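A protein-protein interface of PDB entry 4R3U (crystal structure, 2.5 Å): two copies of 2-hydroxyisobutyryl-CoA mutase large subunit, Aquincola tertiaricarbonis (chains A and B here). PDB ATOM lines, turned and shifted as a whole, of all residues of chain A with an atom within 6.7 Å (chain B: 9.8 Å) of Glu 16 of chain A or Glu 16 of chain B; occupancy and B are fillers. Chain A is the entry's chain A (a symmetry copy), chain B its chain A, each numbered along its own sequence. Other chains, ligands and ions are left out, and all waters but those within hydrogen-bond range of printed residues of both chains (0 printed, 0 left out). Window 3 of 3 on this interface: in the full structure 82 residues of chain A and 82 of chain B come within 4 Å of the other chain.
The side-chain hydroxyl (OG1) of Thr 13 of chain B is in hydrogen-bond range of the side-chain carboxylate (OE1) of Glu 16 of chain A.
N of Glu 16 of chain A is in hydrogen-bond range of O of Trp 14 of chain B (3.2 Å).
The side-chain carboxylate (OE1) of Glu 16 of chain B is in hydrogen-bond range of the side-chain hydroxyl (OG1) of Thr 13 of chain A, 3.1 Å away.
The backbone NH of Glu 16 of chain B sits at hydrogen-bond distance from the backbone carbonyl oxygen of Trp 14 of chain A (3.2 Å).
CD1 of Ile 19 of chain B touches O of Thr 13 of chain A, at 3.5 Å.
Trp 14 of chain A touches Trp 14 of chain B (CZ3 to CZ3, 3.6 Å).
Trp 14 of chain A touches Leu 15 of chain B.
CB of Trp 14 of chain A touches CG2 of Ile 19 of chain B (3.8 Å).
Leu 15 of chain A touches Trp 14 of chain B.
Leu 15 of chain A touches Glu 16 of chain B.
OE1 of Glu 16 of chain A touches O of Leu 15 of chain B (3.5 Å).
Glu 16 of chain B touches Glu 16 of chain A.
Ile 19 of chain A touches Thr 13 of chain B (CD1 to O, 3.5 Å).
Trp 14 of chain B touches Ile 19 of chain A.
Of chain B, only Glu 16 (3.0 Å) and Ile 19 (3.5 Å) come within 4 Å of Thr 13 of chain A.
Of chain B, only Trp 14 (3.9 Å) and Glu 16 (3.5 Å) come within 4 Å of Leu 15 of chain A.
Pro 17 of chain A touches none of the printed residues of chain B.
Of the printed residues of chain A, Trp 14 of chain B touches Trp 14 (3.6 Å), Leu 15 (3.9 Å), Glu 16 (3.2 Å) and Ile 19 (3.8 Å).
Of chain A, only Thr 13 (3.0 Å), Trp 14 (3.2 Å), Leu 15 (3.5 Å) and Glu 16 (3.8 Å) come within 4 Å of Glu 16 of chain B.
Of the printed residues of chain A, Ile 19 of chain B touches Thr 13 (3.5 Å) and Trp 14 (3.8 Å).
Ala 67 of chain B touches none of the printed residues of chain A.
Printed residues of chain A within 4 Å of Leu 71 of chain B: Ile 19 (3.8 Å).
The nearest residue of chain B that does not touch Glu 16 of chain A is Pro 17 of chain B (4.5 Å).
The nearest printed residue of chain B that does not touch Trp 14 of chain A is Ala 63 of chain B (5.6 Å).
Hydrophobic or aromatic side chains of chain A that line the printed part of chain B: Trp 14, Leu 15 and Ile 19.
Hydrophobic or aromatic side chains of chain B within 4 Å of the printed part of chain A: Trp 14, Leu 15, Ile 19 and Leu 71.
Among the printed residues, 15 pairs touch across the chains.
Among the printed residues, no Asp or Glu carboxylate lies within 4 Å of a Lys or Arg side-chain nitrogen of the other chain.
Trp 14 of chain A touches its own counterpart, Trp 14 of chain B.
Trp 14 of chain A touches Leu 15 of chain B, and with the chains exchanged Leu 15 of chain A touches Trp 14 of chain B.
Trp 14 of chain A touches Glu 16 of chain B, and with the chains exchanged Glu 16 of chain A touches Trp 14 of chain B.
Trp 14 of chain A touches Ile 19 of chain B, and with the chains exchanged Ile 19 of chain A touches Trp 14 of chain B.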
ATOM      1  N   THR A  13      -6.820 -16.066 -15.073  1.00  0.00           N
ATOM      2  CA  THR A  13      -6.568 -17.490 -15.335  1.00  0.00           C
ATOM      3  C   THR A  13      -5.103 -17.869 -15.131  1.00  0.00           C
ATOM      4  O   THR A  13      -4.215 -17.229 -15.701  1.00  0.00           O
ATOM      5  CB  THR A  13      -7.124 -17.974 -16.700  1.00  0.00           C
ATOM      6  OG1 THR A  13      -6.247 -17.595 -17.758  1.00  0.00           O
ATOM      7  CG2 THR A  13      -8.559 -17.512 -16.969  1.00  0.00           C
ATOM      8  N   TRP A  14      -4.863 -18.920 -14.320  1.00  0.00           N
ATOM      9  CA  TRP A  14      -3.526 -19.414 -13.980  1.00  0.00           C
ATOM     10  C   TRP A  14      -3.205 -20.724 -14.667  1.00  0.00           C
ATOM     11  O   TRP A  14      -2.031 -21.025 -14.899  1.00  0.00           O
ATOM     12  CB  TRP A  14      -3.391 -19.561 -12.455  1.00  0.00           C
ATOM     13  CG  TRP A  14      -4.460 -20.395 -11.821  1.00  0.00           C
ATOM     14  CD1 TRP A  14      -5.696 -19.978 -11.416  1.00  0.00           C
ATOM     15  CD2 TRP A  14      -4.398 -21.802 -11.546  1.00  0.00           C
ATOM     16  NE1 TRP A  14      -6.416 -21.041 -10.918  1.00  0.00           N
ATOM     17  CE2 TRP A  14      -5.637 -22.171 -10.967  1.00  0.00           C
ATOM     18  CE3 TRP A  14      -3.419 -22.797 -11.749  1.00  0.00           C
ATOM     19  CZ2 TRP A  14      -5.925 -23.490 -10.590  1.00  0.00           C
ATOM     20  CZ3 TRP A  14      -3.699 -24.096 -11.351  1.00  0.00           C
ATOM     21  CH2 TRP A  14      -4.940 -24.433 -10.785  1.00  0.00           C
ATOM     22  N   LEU A  15      -4.253 -21.511 -14.963  1.00  0.00           N
ATOM     23  CA  LEU A  15      -4.135 -22.803 -15.619  1.00  0.00           C
ATOM     24  C   LEU A  15      -4.178 -22.648 -17.146  1.00  0.00           C
ATOM     25  O   LEU A  15      -5.147 -22.095 -17.687  1.00  0.00           O
ATOM     26  CB  LEU A  15      -5.225 -23.783 -15.110  1.00  0.00           C
ATOM     27  CG  LEU A  15      -5.005 -25.280 -15.405  1.00  0.00           C
ATOM     28  CD1 LEU A  15      -3.771 -25.828 -14.670  1.00  0.00           C
ATOM     29  CD2 LEU A  15      -6.237 -26.089 -15.056  1.00  0.00           C
ATOM     30  N   GLU A  16      -3.102 -23.111 -17.831  1.00  0.00           N
ATOM     31  CA  GLU A  16      -2.969 -23.081 -19.292  1.00  0.00           C
ATOM     32  C   GLU A  16      -4.158 -23.848 -19.888  1.00  0.00           C
ATOM     33  O   GLU A  16      -4.371 -25.008 -19.508  1.00  0.00           O
ATOM     34  CB  GLU A  16      -1.656 -23.719 -19.727  1.00  0.00           C
ATOM     35  CG  GLU A  16      -0.437 -22.896 -19.364  1.00  0.00           C
ATOM     36  CD  GLU A  16       0.857 -23.400 -19.969  1.00  0.00           C
ATOM     37  OE1 GLU A  16       1.883 -23.402 -19.251  1.00  0.00           O
ATOM     38  OE2 GLU A  16       0.854 -23.781 -21.164  1.00  0.00           O
ATOM     39  N   PRO A  17      -5.009 -23.205 -20.733  1.00  0.00           N
ATOM     40  CA  PRO A  17      -6.193 -23.913 -21.264  1.00  0.00           C
ATOM     41  C   PRO A  17      -5.892 -25.196 -22.048  1.00  0.00           C
ATOM     42  O   PRO A  17      -6.758 -26.068 -22.117  1.00  0.00           O
ATOM     43  CB  PRO A  17      -6.912 -22.847 -22.095  1.00  0.00           C
ATOM     44  CG  PRO A  17      -6.359 -21.543 -21.616  1.00  0.00           C
ATOM     45  CD  PRO A  17      -4.940 -21.828 -21.259  1.00  0.00           C
ATOM     46  N   GLN A  18      -4.663 -25.332 -22.603  1.00  0.00           N
ATOM     47  CA  GLN A  18      -4.227 -26.535 -23.311  1.00  0.00           C
ATOM     48  C   GLN A  18      -4.085 -27.707 -22.308  1.00  0.00           C
ATOM     49  O   GLN A  18      -4.343 -28.853 -22.673  1.00  0.00           O
ATOM     50  CB  GLN A  18      -2.919 -26.277 -24.068  1.00  0.00           C
ATOM     51  CG  GLN A  18      -2.749 -27.186 -25.285  1.00  0.00           C
ATOM     52  CD  GLN A  18      -1.407 -27.039 -25.965  1.00  0.00           C
ATOM     53  OE1 GLN A  18      -1.322 -26.668 -27.142  1.00  0.00           O
ATOM     54  NE2 GLN A  18      -0.328 -27.362 -25.255  1.00  0.00           N
ATOM     55  N   ILE A  19      -3.707 -27.397 -21.041  1.00  0.00           N
ATOM     56  CA  ILE A  19      -3.596 -28.342 -19.924  1.00  0.00           C
ATOM     57  C   ILE A  19      -4.982 -28.623 -19.284  1.00  0.00           C
ATOM     58  O   ILE A  19      -5.269 -29.790 -18.997  1.00  0.00           O
ATOM     59  CB  ILE A  19      -2.520 -27.896 -18.889  1.00  0.00           C
ATOM     60  CG1 ILE A  19      -1.166 -27.499 -19.565  1.00  0.00           C
ATOM     61  CG2 ILE A  19      -2.323 -28.940 -17.771  1.00  0.00           C
ATOM     62  CD1 ILE A  19      -0.307 -28.636 -20.182  1.00  0.00           C
ATOM     63  N   LYS A  20      -5.843 -27.572 -19.087  1.00  0.00           N
ATOM     64  CA  LYS A  20      -7.203 -27.722 -18.535  1.00  0.00           C
ATOM     65  C   LYS A  20      -8.030 -28.687 -19.390  1.00  0.00           C
ATOM     66  O   LYS A  20      -8.783 -29.502 -18.846  1.00  0.00           O
ATOM     67  CB  LYS A  20      -7.939 -26.369 -18.417  1.00  0.00           C
ATOM     68  CG  LYS A  20      -9.228 -26.456 -17.566  1.00  0.00           C
ATOM     69  CD  LYS A  20     -10.080 -25.181 -17.559  1.00  0.00           C
ATOM     70  CE  LYS A  20     -11.441 -25.442 -16.948  1.00  0.00           C
ATOM     71  NZ  LYS A  20     -12.285 -24.218 -16.874  1.00  0.00           N
ATOM     72  N   SER A  21      -7.871 -28.582 -20.728  1.00  0.00           N
ATOM     73  CA  SER A  21      -8.530 -29.409 -21.731  1.00  0.00           C
ATOM     74  C   SER A  21      -8.058 -30.829 -21.599  1.00  0.00           C
ATOM     75  O   SER A  21      -8.891 -31.734 -21.565  1.00  0.00           O
ATOM     76  CB  SER A  21      -8.232 -28.888 -23.138  1.00  0.00           C
ATOM     77  OG  SER A  21      -8.868 -27.635 -23.345  1.00  0.00           O
ATOM     78  N   THR B  13       4.643 -27.911 -18.888  1.00  0.00           N
ATOM     79  CA  THR B  13       4.296 -26.771 -18.027  1.00  0.00           C
ATOM     80  C   THR B  13       2.793 -26.508 -17.987  1.00  0.00           C
ATOM     81  O   THR B  13       2.160 -26.377 -19.039  1.00  0.00           O
ATOM     82  CB  THR B  13       5.117 -25.491 -18.337  1.00  0.00           C
ATOM     83  OG1 THR B  13       4.588 -24.824 -19.481  1.00  0.00           O
ATOM     84  CG2 THR B  13       6.618 -25.754 -18.487  1.00  0.00           C
ATOM     85  N   TRP B  14       2.232 -26.423 -16.763  1.00  0.00           N
ATOM     86  CA  TRP B  14       0.803 -26.206 -16.522  1.00  0.00           C
ATOM     87  C   TRP B  14       0.511 -24.808 -16.019  1.00  0.00           C
ATOM     88  O   TRP B  14      -0.594 -24.298 -16.227  1.00  0.00           O
ATOM     89  CB  TRP B  14       0.270 -27.254 -15.531  1.00  0.00           C
ATOM     90  CG  TRP B  14       1.037 -27.330 -14.247  1.00  0.00           C
ATOM     91  CD1 TRP B  14       2.171 -28.053 -14.009  1.00  0.00           C
ATOM     92  CD2 TRP B  14       0.739 -26.633 -13.029  1.00  0.00           C
ATOM     93  NE1 TRP B  14       2.609 -27.838 -12.721  1.00  0.00           N
ATOM     94  CE2 TRP B  14       1.738 -26.985 -12.089  1.00  0.00           C
ATOM     95  CE3 TRP B  14      -0.269 -25.725 -12.642  1.00  0.00           C
ATOM     96  CZ2 TRP B  14       1.761 -26.463 -10.789  1.00  0.00           C
ATOM     97  CZ3 TRP B  14      -0.257 -25.230 -11.346  1.00  0.00           C
ATOM     98  CH2 TRP B  14       0.751 -25.593 -10.438  1.00  0.00           C
ATOM     99  N   LEU B  15       1.497 -24.205 -15.335  1.00  0.00           N
ATOM    100  CA  LEU B  15       1.395 -22.867 -14.776  1.00  0.00           C
ATOM    101  C   LEU B  15       1.841 -21.812 -15.798  1.00  0.00           C
ATOM    102  O   LEU B  15       2.974 -21.870 -16.298  1.00  0.00           O
ATOM    103  CB  LEU B  15       2.195 -22.758 -13.452  1.00  0.00           C
ATOM    104  CG  LEU B  15       1.878 -21.551 -12.547  1.00  0.00           C
ATOM    105  CD1 LEU B  15       0.443 -21.611 -12.001  1.00  0.00           C
ATOM    106  CD2 LEU B  15       2.877 -21.447 -11.411  1.00  0.00           C
ATOM    107  N   GLU B  16       0.925 -20.866 -16.129  1.00  0.00           N
ATOM    108  CA  GLU B  16       1.169 -19.759 -17.061  1.00  0.00           C
ATOM    109  C   GLU B  16       2.370 -18.959 -16.535  1.00  0.00           C
ATOM    110  O   GLU B  16       2.339 -18.532 -15.372  1.00  0.00           O
ATOM    111  CB  GLU B  16      -0.058 -18.864 -17.169  1.00  0.00           C
ATOM    112  CG  GLU B  16      -1.221 -19.520 -17.884  1.00  0.00           C
ATOM    113  CD  GLU B  16      -2.371 -18.582 -18.191  1.00  0.00           C
ATOM    114  OE1 GLU B  16      -3.538 -19.004 -18.018  1.00  0.00           O
ATOM    115  OE2 GLU B  16      -2.112 -17.432 -18.617  1.00  0.00           O
ATOM    116  N   PRO B  17       3.478 -18.831 -17.315  1.00  0.00           N
ATOM    117  CA  PRO B  17       4.663 -18.117 -16.796  1.00  0.00           C
ATOM    118  C   PRO B  17       4.418 -16.665 -16.368  1.00  0.00           C
ATOM    119  O   PRO B  17       5.163 -16.159 -15.528  1.00  0.00           O
ATOM    120  CB  PRO B  17       5.691 -18.253 -17.923  1.00  0.00           C
ATOM    121  CG  PRO B  17       5.196 -19.385 -18.766  1.00  0.00           C
ATOM    122  CD  PRO B  17       3.709 -19.303 -18.694  1.00  0.00           C
ATOM    123  N   GLN B  18       3.362 -16.009 -16.908  1.00  0.00           N
ATOM    124  CA  GLN B  18       2.978 -14.650 -16.528  1.00  0.00           C
ATOM    125  C   GLN B  18       2.447 -14.646 -15.073  1.00  0.00           C
ATOM    126  O   GLN B  18       2.650 -13.667 -14.355  1.00  0.00           O
ATOM    127  CB  GLN B  18       1.944 -14.083 -17.508  1.00  0.00           C
ATOM    128  CG  GLN B  18       1.980 -12.557 -17.590  1.00  0.00           C
ATOM    129  CD  GLN B  18       0.881 -11.973 -18.448  1.00  0.00           C
ATOM    130  OE1 GLN B  18       1.141 -11.306 -19.456  1.00  0.00           O
ATOM    131  NE2 GLN B  18      -0.374 -12.177 -18.050  1.00  0.00           N
ATOM    132  N   ILE B  19       1.802 -15.761 -14.644  1.00  0.00           N
ATOM    133  CA  ILE B  19       1.300 -15.991 -13.285  1.00  0.00           C
ATOM    134  C   ILE B  19       2.435 -16.465 -12.338  1.00  0.00           C
ATOM    135  O   ILE B  19       2.499 -15.971 -11.207  1.00  0.00           O
ATOM    136  CB  ILE B  19       0.059 -16.934 -13.276  1.00  0.00           C
ATOM    137  CG1 ILE B  19      -1.022 -16.512 -14.324  1.00  0.00           C
ATOM    138  CG2 ILE B  19      -0.538 -17.092 -11.862  1.00  0.00           C
ATOM    139  CD1 ILE B  19      -1.827 -15.213 -14.047  1.00  0.00           C
ATOM    140  N   LYS B  20       3.339 -17.390 -12.801  1.00  0.00           N
ATOM    141  CA  LYS B  20       4.486 -17.876 -12.012  1.00  0.00           C
ATOM    142  C   LYS B  20       5.381 -16.709 -11.583  1.00  0.00           C
ATOM    143  O   LYS B  20       5.868 -16.691 -10.448  1.00  0.00           O
ATOM    144  CB  LYS B  20       5.326 -18.918 -12.784  1.00  0.00           C
ATOM    145  CG  LYS B  20       6.338 -19.664 -11.882  1.00  0.00           C
ATOM    146  CD  LYS B  20       7.307 -20.587 -12.632  1.00  0.00           C
ATOM    147  CE  LYS B  20       8.428 -21.047 -11.723  1.00  0.00           C
ATOM    148  NZ  LYS B  20       9.367 -21.987 -12.395  1.00  0.00           N
ATOM    149  N   SER B  21       5.578 -15.741 -12.505  1.00  0.00           N
ATOM    150  CA  SER B  21       6.366 -14.529 -12.312  1.00  0.00           C
ATOM    151  C   SER B  21       5.709 -13.665 -11.273  1.00  0.00           C
ATOM    152  O   SER B  21       6.391 -13.212 -10.355  1.00  0.00           O
ATOM    153  CB  SER B  21       6.497 -13.758 -13.626  1.00  0.00           C
ATOM    154  OG  SER B  21       7.311 -14.477 -14.541  1.00  0.00           O
ATOM    155  N   GLN B  22       4.377 -13.454 -11.404  1.00  0.00           N
ATOM    156  CA  GLN B  22       3.559 -12.683 -10.469  1.00  0.00           C
ATOM    157  C   GLN B  22       3.686 -13.272  -9.062  1.00  0.00           C
ATOM    158  O   GLN B  22       3.996 -12.531  -8.132  1.00  0.00           O
ATOM    159  CB  GLN B  22       2.083 -12.697 -10.901  1.00  0.00           C
ATOM    160  CG  GLN B  22       1.680 -11.552 -11.825  1.00  0.00           C
ATOM    161  CD  GLN B  22       0.224 -11.658 -12.234  1.00  0.00           C
ATOM    162  OE1 GLN B  22      -0.677 -11.945 -11.421  1.00  0.00           O
ATOM    163  NE2 GLN B  22      -0.042 -11.409 -13.509  1.00  0.00           N
ATOM    164  N   LEU B  23       3.508 -14.604  -8.926  1.00  0.00           N
ATOM    165  CA  LEU B  23       3.605 -15.315  -7.649  1.00  0.00           C
ATOM    166  C   LEU B  23       4.941 -15.096  -6.964  1.00  0.00           C
ATOM    167  O   LEU B  23       4.953 -14.759  -5.778  1.00  0.00           O
ATOM    168  CB  LEU B  23       3.354 -16.833  -7.813  1.00  0.00           C
ATOM    169  CG  LEU B  23       1.938 -17.280  -8.158  1.00  0.00           C
ATOM    170  CD1 LEU B  23       1.922 -18.741  -8.538  1.00  0.00           C
ATOM    171  CD2 LEU B  23       0.997 -17.038  -7.013  1.00  0.00           C
ATOM    172  N   GLN B  24       6.056 -15.276  -7.706  1.00  0.00           N
ATOM    173  CA  GLN B  24       7.419 -15.134  -7.191  1.00  0.00           C
ATOM    174  C   GLN B  24       7.740 -13.686  -6.808  1.00  0.00           C
ATOM    175  O   GLN B  24       8.448 -13.454  -5.831  1.00  0.00           O
ATOM    176  CB  GLN B  24       8.449 -15.681  -8.201  1.00  0.00           C
ATOM    177  CG  GLN B  24       8.493 -17.207  -8.312  1.00  0.00           C
ATOM    178  CD  GLN B  24       9.375 -17.650  -9.461  1.00  0.00           C
ATOM    179  OE1 GLN B  24       8.973 -17.638 -10.630  1.00  0.00           O
ATOM    180  NE2 GLN B  24      10.610 -18.036  -9.161  1.00  0.00           N
ATOM    181  N   ALA B  63       1.786 -22.020  -5.858  1.00  0.00           N
ATOM    182  CA  ALA B  63       1.745 -22.809  -7.094  1.00  0.00           C
ATOM    183  C   ALA B  63       3.082 -22.782  -7.823  1.00  0.00           C
ATOM    184  O   ALA B  63       3.390 -23.736  -8.543  1.00  0.00           O
ATOM    185  CB  ALA B  63       0.648 -22.297  -8.002  1.00  0.00           C
ATOM    186  N   ALA B  64       3.888 -21.702  -7.603  1.00  0.00           N
ATOM    187  CA  ALA B  64       5.205 -21.505  -8.204  1.00  0.00           C
ATOM    188  C   ALA B  64       6.182 -22.627  -7.809  1.00  0.00           C
ATOM    189  O   ALA B  64       6.972 -23.097  -8.643  1.00  0.00           O
ATOM    190  CB  ALA B  64       5.761 -20.137  -7.824  1.00  0.00           C
ATOM    191  N   ALA B  67       5.395 -25.774  -9.999  1.00  0.00           N
ATOM    192  CA  ALA B  67       5.348 -25.512 -11.445  1.00  0.00           C
ATOM    193  C   ALA B  67       6.267 -26.435 -12.253  1.00  0.00           C
ATOM    194  O   ALA B  67       5.934 -26.769 -13.389  1.00  0.00           O
ATOM    195  CB  ALA B  67       5.698 -24.055 -11.727  1.00  0.00           C
ATOM    196  N   LEU B  71       1.705 -32.045 -14.265  1.00  0.00           N
ATOM    197  CA  LEU B  71       0.448 -32.554 -13.734  1.00  0.00           C
ATOM    198  C   LEU B  71       0.231 -34.039 -13.969  1.00  0.00           C
ATOM    199  O   LEU B  71      -0.500 -34.652 -13.197  1.00  0.00           O
ATOM    200  CB  LEU B  71      -0.730 -31.707 -14.195  1.00  0.00           C
ATOM    201  CG  LEU B  71      -0.803 -30.285 -13.631  1.00  0.00           C
ATOM    202  CD1 LEU B  71      -2.096 -29.638 -14.027  1.00  0.00           C
ATOM    203  CD2 LEU B  71      -0.639 -30.267 -12.099  1.00  0.00           C
